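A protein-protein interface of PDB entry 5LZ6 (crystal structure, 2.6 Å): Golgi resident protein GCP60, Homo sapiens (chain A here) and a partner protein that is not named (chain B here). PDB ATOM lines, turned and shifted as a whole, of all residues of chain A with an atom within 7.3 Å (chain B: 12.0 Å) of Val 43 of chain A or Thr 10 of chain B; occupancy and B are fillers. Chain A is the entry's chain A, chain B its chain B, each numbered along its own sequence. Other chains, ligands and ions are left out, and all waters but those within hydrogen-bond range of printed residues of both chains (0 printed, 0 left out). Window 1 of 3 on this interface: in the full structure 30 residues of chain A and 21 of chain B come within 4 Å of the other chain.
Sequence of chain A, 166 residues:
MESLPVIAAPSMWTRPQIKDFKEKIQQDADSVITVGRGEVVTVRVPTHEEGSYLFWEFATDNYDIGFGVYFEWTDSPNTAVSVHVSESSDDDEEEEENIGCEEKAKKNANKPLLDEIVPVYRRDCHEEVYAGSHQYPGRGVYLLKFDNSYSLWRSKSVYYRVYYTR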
ATOM      1  N   ASP A  30       5.085  12.937 -12.150  1.00  0.00           N
ATOM      2  CA  ASP A  30       5.331  11.712 -12.905  1.00  0.00           C
ATOM      3  C   ASP A  30       4.283  10.635 -12.624  1.00  0.00           C
ATOM      4  O   ASP A  30       4.392   9.515 -13.124  1.00  0.00           O
ATOM      5  CB  ASP A  30       6.725  11.167 -12.586  1.00  0.00           C
ATOM      6  N   SER A  31       3.274  10.979 -11.827  1.00  0.00           N
ATOM      7  CA  SER A  31       2.221  10.038 -11.463  1.00  0.00           C
ATOM      8  C   SER A  31       0.882  10.386 -12.117  1.00  0.00           C
ATOM      9  O   SER A  31      -0.120   9.709 -11.882  1.00  0.00           O
ATOM     10  CB  SER A  31       2.058   9.995  -9.943  1.00  0.00           C
ATOM     11  OG  SER A  31       3.276   9.654  -9.306  1.00  0.00           O
ATOM     12  N   ILE A  33      -1.213  11.264 -15.797  1.00  0.00           N
ATOM     13  CA  ILE A  33      -1.235  11.147 -17.253  1.00  0.00           C
ATOM     14  C   ILE A  33      -2.481  11.818 -17.818  1.00  0.00           C
ATOM     15  O   ILE A  33      -3.555  11.761 -17.216  1.00  0.00           O
ATOM     16  CB  ILE A  33      -1.204   9.669 -17.709  1.00  0.00           C
ATOM     17  CG1 ILE A  33       0.071   8.986 -17.216  1.00  0.00           C
ATOM     18  CG2 ILE A  33      -1.297   9.564 -19.233  1.00  0.00           C
ATOM     19  CD1 ILE A  33       0.082   7.481 -17.418  1.00  0.00           C
ATOM     20  N   VAL A  41      -2.628   5.005 -24.084  1.00  0.00           N
ATOM     21  CA  VAL A  41      -1.317   5.114 -23.450  1.00  0.00           C
ATOM     22  C   VAL A  41      -0.946   3.803 -22.768  1.00  0.00           C
ATOM     23  O   VAL A  41      -1.722   3.265 -21.976  1.00  0.00           O
ATOM     24  CB  VAL A  41      -1.282   6.256 -22.414  1.00  0.00           C
ATOM     25  CG1 VAL A  41       0.115   6.401 -21.822  1.00  0.00           C
ATOM     26  CG2 VAL A  41      -1.723   7.563 -23.051  1.00  0.00           C
ATOM     27  N   THR A  42       0.244   3.299 -23.082  1.00  0.00           N
ATOM     28  CA  THR A  42       0.770   2.096 -22.451  1.00  0.00           C
ATOM     29  C   THR A  42       1.891   2.460 -21.488  1.00  0.00           C
ATOM     30  O   THR A  42       2.881   3.075 -21.880  1.00  0.00           O
ATOM     31  CB  THR A  42       1.303   1.090 -23.490  1.00  0.00           C
ATOM     32  OG1 THR A  42       0.267   0.767 -24.424  1.00  0.00           O
ATOM     33  CG2 THR A  42       1.788  -0.189 -22.811  1.00  0.00           C
ATOM     34  N   VAL A  43       1.725   2.080 -20.227  1.00  0.00           N
ATOM     35  CA  VAL A  43       2.774   2.259 -19.235  1.00  0.00           C
ATOM     36  C   VAL A  43       3.539   0.951 -19.075  1.00  0.00           C
ATOM     37  O   VAL A  43       2.971  -0.070 -18.686  1.00  0.00           O
ATOM     38  CB  VAL A  43       2.210   2.700 -17.874  1.00  0.00           C
ATOM     39  CG1 VAL A  43       3.344   3.051 -16.924  1.00  0.00           C
ATOM     40  CG2 VAL A  43       1.280   3.889 -18.047  1.00  0.00           C
ATOM     41  N   ARG A  44       4.828   0.988 -19.389  1.00  0.00           N
ATOM     42  CA  ARG A  44       5.684  -0.180 -19.244  1.00  0.00           C
ATOM     43  C   ARG A  44       6.257  -0.231 -17.831  1.00  0.00           C
ATOM     44  O   ARG A  44       6.860   0.734 -17.360  1.00  0.00           O
ATOM     45  CB  ARG A  44       6.803  -0.151 -20.286  1.00  0.00           C
ATOM     46  CG  ARG A  44       6.294  -0.097 -21.720  1.00  0.00           C
ATOM     47  CD  ARG A  44       7.434  -0.070 -22.725  1.00  0.00           C
ATOM     48  NE  ARG A  44       8.332  -1.211 -22.562  1.00  0.00           N
ATOM     49  CZ  ARG A  44       8.142  -2.407 -23.111  1.00  0.00           C
ATOM     50  NH1 ARG A  44       7.080  -2.641 -23.874  1.00  0.00           N
ATOM     51  NH2 ARG A  44       9.019  -3.376 -22.895  1.00  0.00           N
ATOM     52  N   VAL A  45       6.047  -1.358 -17.157  1.00  0.00           N
ATOM     53  CA  VAL A  45       6.496  -1.538 -15.779  1.00  0.00           C
ATOM     54  C   VAL A  45       7.335  -2.807 -15.667  1.00  0.00           C
ATOM     55  O   VAL A  45       6.790  -3.902 -15.531  1.00  0.00           O
ATOM     56  CB  VAL A  45       5.306  -1.619 -14.802  1.00  0.00           C
ATOM     57  CG1 VAL A  45       5.794  -1.671 -13.360  1.00  0.00           C
ATOM     58  CG2 VAL A  45       4.382  -0.434 -15.000  1.00  0.00           C
ATOM     59  N   PRO A  46       8.670  -2.665 -15.730  1.00  0.00           N
ATOM     60  CA  PRO A  46       9.550  -3.835 -15.640  1.00  0.00           C
ATOM     61  C   PRO A  46       9.454  -4.548 -14.298  1.00  0.00           C
ATOM     62  O   PRO A  46       9.314  -3.901 -13.259  1.00  0.00           O
ATOM     63  CB  PRO A  46      10.950  -3.242 -15.830  1.00  0.00           C
ATOM     64  CG  PRO A  46      10.737  -1.924 -16.476  1.00  0.00           C
ATOM     65  CD  PRO A  46       9.432  -1.426 -15.956  1.00  0.00           C
ATOM     66  N   TYR A  70      -1.204  -6.462 -19.570  1.00  0.00           N
ATOM     67  CA  TYR A  70      -0.549  -7.520 -20.327  1.00  0.00           C
ATOM     68  C   TYR A  70       0.850  -7.738 -19.773  1.00  0.00           C
ATOM     69  O   TYR A  70       1.401  -6.860 -19.110  1.00  0.00           O
ATOM     70  CB  TYR A  70      -0.482  -7.170 -21.815  1.00  0.00           C
ATOM     71  CG  TYR A  70      -1.820  -7.191 -22.516  1.00  0.00           C
ATOM     72  CD1 TYR A  70      -2.261  -8.331 -23.173  1.00  0.00           C
ATOM     73  CD2 TYR A  70      -2.638  -6.071 -22.525  1.00  0.00           C
ATOM     74  CE1 TYR A  70      -3.483  -8.356 -23.818  1.00  0.00           C
ATOM     75  CE2 TYR A  70      -3.861  -6.087 -23.166  1.00  0.00           C
ATOM     76  CZ  TYR A  70      -4.278  -7.232 -23.812  1.00  0.00           C
ATOM     77  OH  TYR A  70      -5.496  -7.251 -24.451  1.00  0.00           O
ATOM     78  N   VAL A 141       8.079  -7.404 -18.626  1.00  0.00           N
ATOM     79  CA  VAL A 141       7.548  -6.049 -18.556  1.00  0.00           C
ATOM     80  C   VAL A 141       6.025  -6.080 -18.597  1.00  0.00           C
ATOM     81  O   VAL A 141       5.430  -6.567 -19.560  1.00  0.00           O
ATOM     82  CB  VAL A 141       8.073  -5.172 -19.720  1.00  0.00           C
ATOM     83  CG1 VAL A 141       7.507  -3.759 -19.640  1.00  0.00           C
ATOM     84  CG2 VAL A 141       9.596  -5.126 -19.719  1.00  0.00           C
ATOM     85  N   TYR A 142       5.398  -5.560 -17.548  1.00  0.00           N
ATOM     86  CA  TYR A 142       3.950  -5.415 -17.525  1.00  0.00           C
ATOM     87  C   TYR A 142       3.527  -4.233 -18.380  1.00  0.00           C
ATOM     88  O   TYR A 142       4.172  -3.183 -18.363  1.00  0.00           O
ATOM     89  CB  TYR A 142       3.442  -5.231 -16.097  1.00  0.00           C
ATOM     90  CG  TYR A 142       3.373  -6.508 -15.299  1.00  0.00           C
ATOM     91  CD1 TYR A 142       2.272  -7.348 -15.393  1.00  0.00           C
ATOM     92  CD2 TYR A 142       4.399  -6.864 -14.438  1.00  0.00           C
ATOM     93  CE1 TYR A 142       2.202  -8.516 -14.656  1.00  0.00           C
ATOM     94  CE2 TYR A 142       4.337  -8.024 -13.699  1.00  0.00           C
ATOM     95  CZ  TYR A 142       3.239  -8.846 -13.810  1.00  0.00           C
ATOM     96  OH  TYR A 142       3.192 -10.001 -13.067  1.00  0.00           O
ATOM     97  N   LEU A 143       2.441  -4.410 -19.126  1.00  0.00           N
ATOM     98  CA  LEU A 143       1.892  -3.350 -19.960  1.00  0.00           C
ATOM     99  C   LEU A 143       0.526  -2.921 -19.448  1.00  0.00           C
ATOM    100  O   LEU A 143      -0.473  -3.601 -19.685  1.00  0.00           O
ATOM    101  CB  LEU A 143       1.782  -3.808 -21.415  1.00  0.00           C
ATOM    102  CG  LEU A 143       3.070  -4.289 -22.083  1.00  0.00           C
ATOM    103  CD1 LEU A 143       2.777  -4.734 -23.505  1.00  0.00           C
ATOM    104  CD2 LEU A 143       4.134  -3.205 -22.066  1.00  0.00           C
ATOM    105  N   LEU A 144       0.486  -1.795 -18.744  1.00  0.00           N
ATOM    106  CA  LEU A 144      -0.772  -1.242 -18.268  1.00  0.00           C
ATOM    107  C   LEU A 144      -1.383  -0.362 -19.350  1.00  0.00           C
ATOM    108  O   LEU A 144      -0.839   0.688 -19.693  1.00  0.00           O
ATOM    109  CB  LEU A 144      -0.568  -0.451 -16.974  1.00  0.00           C
ATOM    110  CG  LEU A 144      -0.583  -1.300 -15.698  1.00  0.00           C
ATOM    111  CD1 LEU A 144       0.610  -2.247 -15.648  1.00  0.00           C
ATOM    112  CD2 LEU A 144      -0.618  -0.413 -14.463  1.00  0.00           C
ATOM    113  N   LYS A 145      -2.511  -0.811 -19.892  1.00  0.00           N
ATOM    114  CA  LYS A 145      -3.180  -0.114 -20.982  1.00  0.00           C
ATOM    115  C   LYS A 145      -4.242   0.844 -20.455  1.00  0.00           C
ATOM    116  O   LYS A 145      -5.200   0.420 -19.807  1.00  0.00           O
ATOM    117  CB  LYS A 145      -3.824  -1.119 -21.942  1.00  0.00           C
ATOM    118  CG  LYS A 145      -2.843  -2.062 -22.625  1.00  0.00           C
ATOM    119  CD  LYS A 145      -2.033  -1.352 -23.697  1.00  0.00           C
ATOM    120  CE  LYS A 145      -1.231  -2.340 -24.530  1.00  0.00           C
ATOM    121  NZ  LYS A 145      -0.441  -1.671 -25.602  1.00  0.00           N
ATOM    122  N   PHE A 146      -4.059   2.133 -20.728  1.00  0.00           N
ATOM    123  CA  PHE A 146      -5.079   3.136 -20.442  1.00  0.00           C
ATOM    124  C   PHE A 146      -5.730   3.561 -21.754  1.00  0.00           C
ATOM    125  O   PHE A 146      -5.228   4.430 -22.466  1.00  0.00           O
ATOM    126  CB  PHE A 146      -4.478   4.333 -19.704  1.00  0.00           C
ATOM    127  CG  PHE A 146      -4.035   4.014 -18.303  1.00  0.00           C
ATOM    128  CD1 PHE A 146      -4.968   3.794 -17.303  1.00  0.00           C
ATOM    129  CD2 PHE A 146      -2.689   3.928 -17.985  1.00  0.00           C
ATOM    130  CE1 PHE A 146      -4.568   3.497 -16.014  1.00  0.00           C
ATOM    131  CE2 PHE A 146      -2.284   3.631 -16.697  1.00  0.00           C
ATOM    132  CZ  PHE A 146      -3.225   3.416 -15.710  1.00  0.00           C
ATOM    133  N   VAL A 158      -5.492  10.860 -15.668  1.00  0.00           N
ATOM    134  CA  VAL A 158      -5.226   9.584 -15.010  1.00  0.00           C
ATOM    135  C   VAL A 158      -4.182   9.725 -13.907  1.00  0.00           C
ATOM    136  O   VAL A 158      -3.052  10.137 -14.158  1.00  0.00           O
ATOM    137  CB  VAL A 158      -4.751   8.523 -16.038  1.00  0.00           C
ATOM    138  CG1 VAL A 158      -4.218   7.259 -15.352  1.00  0.00           C
ATOM    139  CG2 VAL A 158      -5.880   8.170 -16.985  1.00  0.00           C
ATOM    140  N   TYR A 160      -2.092   7.456 -11.129  1.00  0.00           N
ATOM    141  CA  TYR A 160      -1.718   6.051 -10.997  1.00  0.00           C
ATOM    142  C   TYR A 160      -0.414   5.826 -10.231  1.00  0.00           C
ATOM    143  O   TYR A 160       0.466   6.688 -10.200  1.00  0.00           O
ATOM    144  CB  TYR A 160      -1.602   5.413 -12.383  1.00  0.00           C
ATOM    145  CG  TYR A 160      -0.292   5.701 -13.084  1.00  0.00           C
ATOM    146  CD1 TYR A 160      -0.041   6.942 -13.652  1.00  0.00           C
ATOM    147  CD2 TYR A 160       0.693   4.725 -13.183  1.00  0.00           C
ATOM    148  CE1 TYR A 160       1.156   7.207 -14.291  1.00  0.00           C
ATOM    149  CE2 TYR A 160       1.890   4.979 -13.823  1.00  0.00           C
ATOM    150  CZ  TYR A 160       2.117   6.221 -14.375  1.00  0.00           C
ATOM    151  OH  TYR A 160       3.309   6.476 -15.011  1.00  0.00           O
ATOM    152  N   ARG A 161      -0.315   4.649  -9.620  1.00  0.00           N
ATOM    153  CA  ARG A 161       0.898   4.195  -8.944  1.00  0.00           C
ATOM    154  C   ARG A 161       1.129   2.718  -9.257  1.00  0.00           C
ATOM    155  O   ARG A 161       0.178   1.937  -9.295  1.00  0.00           O
ATOM    156  CB  ARG A 161       0.792   4.398  -7.429  1.00  0.00           C
ATOM    157  CG  ARG A 161       0.944   5.839  -6.955  1.00  0.00           C
ATOM    158  CD  ARG A 161       2.311   6.088  -6.328  1.00  0.00           C
ATOM    159  NE  ARG A 161       2.350   7.337  -5.566  1.00  0.00           N
ATOM    160  CZ  ARG A 161       2.055   7.445  -4.272  1.00  0.00           C
ATOM    161  NH1 ARG A 161       1.694   6.379  -3.565  1.00  0.00           N
ATOM    162  NH2 ARG A 161       2.123   8.628  -3.678  1.00  0.00           N
ATOM    163  N   VAL A 162       2.386   2.343  -9.489  1.00  0.00           N
ATOM    164  CA  VAL A 162       2.758   0.941  -9.684  1.00  0.00           C
ATOM    165  C   VAL A 162       3.833   0.546  -8.676  1.00  0.00           C
ATOM    166  O   VAL A 162       4.683   1.366  -8.323  1.00  0.00           O
ATOM    167  CB  VAL A 162       3.262   0.673 -11.122  1.00  0.00           C
ATOM    168  CG1 VAL A 162       2.113   0.787 -12.110  1.00  0.00           C
ATOM    169  CG2 VAL A 162       4.393   1.626 -11.493  1.00  0.00           C
ATOM    170  N   SER B   4      -4.371   6.901 -32.507  1.00  0.00           N
ATOM    171  CA  SER B   4      -3.316   7.568 -31.751  1.00  0.00           C
ATOM    172  C   SER B   4      -2.809   6.693 -30.606  1.00  0.00           C
ATOM    173  O   SER B   4      -3.589   6.005 -29.946  1.00  0.00           O
ATOM    174  CB  SER B   4      -3.819   8.900 -31.198  1.00  0.00           C
ATOM    175  OG  SER B   4      -2.795   9.568 -30.482  1.00  0.00           O
ATOM    176  N   GLU B   5      -1.499   6.734 -30.373  1.00  0.00           N
ATOM    177  CA  GLU B   5      -0.869   5.900 -29.353  1.00  0.00           C
ATOM    178  C   GLU B   5       0.296   6.600 -28.663  1.00  0.00           C
ATOM    179  O   GLU B   5       0.922   7.500 -29.224  1.00  0.00           O
ATOM    180  CB  GLU B   5      -0.373   4.592 -29.971  1.00  0.00           C
ATOM    181  CG  GLU B   5      -1.464   3.568 -30.223  1.00  0.00           C
ATOM    182  CD  GLU B   5      -0.948   2.337 -30.942  1.00  0.00           C
ATOM    183  OE1 GLU B   5      -1.718   1.732 -31.717  1.00  0.00           O
ATOM    184  OE2 GLU B   5       0.228   1.973 -30.731  1.00  0.00           O
ATOM    185  N   ARG B   6       0.574   6.167 -27.438  1.00  0.00           N
ATOM    186  CA  ARG B   6       1.716   6.648 -26.671  1.00  0.00           C
ATOM    187  C   ARG B   6       2.260   5.515 -25.812  1.00  0.00           C
ATOM    188  O   ARG B   6       1.549   4.550 -25.527  1.00  0.00           O
ATOM    189  CB  ARG B   6       1.324   7.834 -25.789  1.00  0.00           C
ATOM    190  CG  ARG B   6       1.950   9.154 -26.197  1.00  0.00           C
ATOM    191  CD  ARG B   6       1.882  10.158 -25.057  1.00  0.00           C
ATOM    192  NE  ARG B   6       0.506  10.457 -24.671  1.00  0.00           N
ATOM    193  CZ  ARG B   6       0.141  10.943 -23.487  1.00  0.00           C
ATOM    194  NH1 ARG B   6       1.047  11.184 -22.549  1.00  0.00           N
ATOM    195  NH2 ARG B   6      -1.138  11.183 -23.238  1.00  0.00           N
ATOM    196  N   THR B   7       3.519   5.631 -25.403  1.00  0.00           N
ATOM    197  CA  THR B   7       4.140   4.617 -24.558  1.00  0.00           C
ATOM    198  C   THR B   7       5.337   5.188 -23.807  1.00  0.00           C
ATOM    199  O   THR B   7       6.151   5.914 -24.377  1.00  0.00           O
ATOM    200  CB  THR B   7       4.605   3.393 -25.384  1.00  0.00           C
ATOM    201  OG1 THR B   7       3.492   2.839 -26.098  1.00  0.00           O
ATOM    202  CG2 THR B   7       5.205   2.316 -24.479  1.00  0.00           C
ATOM    203  N   PHE B   8       5.433   4.855 -22.524  1.00  0.00           N
ATOM    204  CA  PHE B   8       6.614   5.188 -21.735  1.00  0.00           C
ATOM    205  C   PHE B   8       6.736   4.265 -20.528  1.00  0.00           C
ATOM    206  O   PHE B   8       5.785   3.574 -20.160  1.00  0.00           O
ATOM    207  CB  PHE B   8       6.579   6.649 -21.285  1.00  0.00           C
ATOM    208  CG  PHE B   8       5.351   7.018 -20.509  1.00  0.00           C
ATOM    209  CD1 PHE B   8       4.225   7.496 -21.158  1.00  0.00           C
ATOM    210  CD2 PHE B   8       5.324   6.901 -19.129  1.00  0.00           C
ATOM    211  CE1 PHE B   8       3.094   7.843 -20.450  1.00  0.00           C
ATOM    212  CE2 PHE B   8       4.195   7.246 -18.415  1.00  0.00           C
ATOM    213  CZ  PHE B   8       3.079   7.718 -19.075  1.00  0.00           C
ATOM    214  N   GLU B   9       7.918   4.267 -19.918  1.00  0.00           N
ATOM    215  CA  GLU B   9       8.238   3.351 -18.830  1.00  0.00           C
ATOM    216  C   GLU B   9       8.134   4.038 -17.471  1.00  0.00           C
ATOM    217  O   GLU B   9       8.391   5.236 -17.350  1.00  0.00           O
ATOM    218  CB  GLU B   9       9.644   2.777 -19.031  1.00  0.00           C
ATOM    219  CG  GLU B   9      10.145   1.897 -17.892  1.00  0.00           C
ATOM    220  CD  GLU B   9      11.494   1.261 -18.193  1.00  0.00           C
ATOM    221  OE1 GLU B   9      11.852   1.152 -19.385  1.00  0.00           O
ATOM    222  OE2 GLU B   9      12.198   0.875 -17.237  1.00  0.00           O
ATOM    223  N   THR B  10       7.750   3.269 -16.457  1.00  0.00           N
ATOM    224  CA  THR B  10       7.665   3.774 -15.090  1.00  0.00           C
ATOM    225  C   THR B  10       8.165   2.721 -14.108  1.00  0.00           C
ATOM    226  O   THR B  10       7.661   1.598 -14.074  1.00  0.00           O
ATOM    227  CB  THR B  10       6.224   4.176 -14.722  1.00  0.00           C
ATOM    228  OG1 THR B  10       5.735   5.132 -15.671  1.00  0.00           O
ATOM    229  CG2 THR B  10       6.167   4.782 -13.324  1.00  0.00           C
ATOM    230  N   ALA B  11       9.157   3.094 -13.308  1.00  0.00           N
ATOM    231  CA  ALA B  11       9.752   2.177 -12.343  1.00  0.00           C
ATOM    232  C   ALA B  11       8.797   1.913 -11.180  1.00  0.00           C
ATOM    233  O   ALA B  11       8.271   2.855 -10.586  1.00  0.00           O
ATOM    234  CB  ALA B  11      11.064   2.737 -11.828  1.00  0.00           C
ATOM    235  N   PRO B  12       8.568   0.630 -10.848  1.00  0.00           N
ATOM    236  CA  PRO B  12       7.704   0.335  -9.702  1.00  0.00           C
ATOM    237  C   PRO B  12       8.388   0.616  -8.369  1.00  0.00           C
ATOM    238  O   PRO B  12       9.557   0.273  -8.195  1.00  0.00           O
ATOM    239  CB  PRO B  12       7.411  -1.159  -9.863  1.00  0.00           C
ATOM    240  CG  PRO B  12       8.595  -1.692 -10.576  1.00  0.00           C
ATOM    241  CD  PRO B  12       9.045  -0.600 -11.506  1.00  0.00           C
ATOM    242  N   SER B  13       7.662   1.237  -7.445  1.00  0.00           N
ATOM    243  CA  SER B  13       8.182   1.514  -6.110  1.00  0.00           C
ATOM    244  C   SER B  13       7.950   0.316  -5.196  1.00  0.00           C
ATOM    245  O   SER B  13       7.056  -0.489  -5.440  1.00  0.00           O
ATOM    246  CB  SER B  13       7.515   2.759  -5.522  1.00  0.00           C
ATOM    247  OG  SER B  13       7.615   3.856  -6.412  1.00  0.00           O
ATOM    248  N   GLU B  14       8.751   0.189  -4.146  1.00  0.00           N
ATOM    249  CA  GLU B  14       8.550  -0.895  -3.197  1.00  0.00           C
ATOM    250  C   GLU B  14       7.335  -0.585  -2.337  1.00  0.00           C
ATOM    251  O   GLU B  14       7.168   0.544  -1.877  1.00  0.00           O
ATOM    252  CB  GLU B  14       9.782  -1.104  -2.318  1.00  0.00           C
ATOM    253  CG  GLU B  14       9.692  -2.346  -1.441  1.00  0.00           C
ATOM    254  CD  GLU B  14      10.902  -2.526  -0.544  1.00  0.00           C
ATOM    255  OE1 GLU B  14      11.660  -1.551  -0.357  1.00  0.00           O
ATOM    256  OE2 GLU B  14      11.096  -3.647  -0.026  1.00  0.00           O
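O of Arg 6 of chain B is in hydrogen-bond range of N of Thr 42 of chain A (3.0 Å).
The backbone carbonyl oxygen (O) of Thr 42 of chain A is in hydrogen-bond range of the backbone NH (N) of Phe 8 of chain B, 3.2 Å away.
The backbone carbonyl oxygen (O) of Phe 8 of chain B sits at hydrogen-bond distance from the backbone NH (N) of Arg 44 of chain A (2.9 Å).
N of Thr 10 of chain B lies within hydrogen-bond range of O of Arg 44 of chain A (2.8 Å).
OH of Tyr 160 of chain A lies within hydrogen-bond range of OG1 of Thr 10 of chain B, 2.9 Å away.
The backbone NH of Ser 13 of chain B sits at hydrogen-bond distance from the backbone carbonyl oxygen of Val 162 of chain A.
N of Tyr 160 of chain A sits at hydrogen-bond distance from O of Ser 31 of chain A, 3.1 Å away.
The backbone carbonyl oxygen (O) of Ile 33 of chain A lies within hydrogen-bond range of the backbone NH (N) of Val 158 of chain A.
The backbone NH of Phe 146 of chain A sits at hydrogen-bond distance from the backbone carbonyl oxygen of Val 41 of chain A (2.9 Å).
The side-chain amino group (NZ) of Lys 145 of chain A lies within hydrogen-bond range of the side-chain hydroxyl (OG1) of Thr 42 of chain A.
N of Val 43 of chain A sits at hydrogen-bond distance from O of Leu 144 of chain A (3.0 Å).
The backbone NH of Val 45 of chain A lies within hydrogen-bond range of the backbone carbonyl oxygen of Tyr 142 of chain A.
Among the printed residues, merely in contact across the chains: Ile 33 of chain A with Phe 8 of chain B, Val 41 of chain A with Arg 6 of chain B, Val 41 of chain A with Phe 8 of chain B, Thr 42 of chain A with Thr 7 of chain B, Val 43 of chain A with Phe 8 of chain B, Val 43 of chain A with Thr 10 of chain B, Arg 44 of chain A with Thr 7 of chain B, Arg 44 of chain A with Glu 9 of chain B, Val 45 of chain A with Thr 10 of chain B, Val 45 of chain A with Pro 12 of chain B, Pro 46 of chain A with Glu 9 of chain B, Pro 46 of chain A with Thr 10 of chain B, Pro 46 of chain A with Pro 12 of chain B, Tyr 160 of chain A with Phe 8 of chain B and Val 162 of chain A with Pro 12 of chain B.
Printed residues of chain B within 4 Å of Val 43 of chain A: Phe 8 (3.4 Å) and Thr 10 (3.4 Å).
Of chain A, only Val 43 (3.4 Å), Arg 44 (2.8 Å), Val 45 (3.8 Å), Pro 46 (3.98 Å) and Tyr 160 (2.9 Å) come within 4 Å of Thr 10 of chain B.
Thr 42 of chain A touches just these residues of chain B: Arg 6, Thr 7 and Phe 8.
Val 45 of chain A touches just these residues of chain B: Thr 10 and Pro 12.
Pro 46 of chain A touches just these residues of chain B: Glu 9, Thr 10 and Pro 12.
No residue of chain B comes within 4 Å of Leu 143 of chain A.
No residue of chain B comes within 4 Å of Leu 144 of chain A.
No residue of chain B comes within 4 Å of Phe 146 of chain A.
Of the printed residues of chain B, Tyr 160 of chain A touches Phe 8 (3.6 Å) and Thr 10 (2.9 Å).
Printed residues of chain B within 4 Å of Arg 44 of chain A: Thr 7, Phe 8, Glu 9 and Thr 10.
Of the printed residues of chain A, Thr 7 of chain B touches Thr 42 and Arg 44.
Of the printed residues of chain A, Pro 12 of chain B touches Val 45 (3.9 Å), Pro 46 (3.5 Å) and Val 162 (3.5 Å).
Of the printed residues of chain A, Arg 6 of chain B touches Val 41 (3.6 Å) and Thr 42 (3.0 Å).
Asp 30 of chain A touches none of the printed residues of chain B.
The nearest residue of chain B that does not touch Val 43 of chain A is Glu 9 of chain B (4.9 Å).
The nearest residue of chain A that does not touch Thr 10 of chain B is Val 162 of chain A (4.1 Å).
The nearest printed residue of chain A that does not touch Pro 12 of chain B is Arg 44 of chain A (6.4 Å).
Hydrophobic or aromatic side chains of chain B within 4 Å of the printed part of chain A: Phe 8 and Pro 12.
Hydrophobic or aromatic side chains of chain A within 4 Å of the printed part of chain B: Ile 33, Val 41, Val 43, Val 45, Pro 46, Tyr 160 and Val 162.
Among the printed residues, no Asp or Glu carboxylate lies within 4 Å of a Lys or Arg side-chain nitrogen of the other chain.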
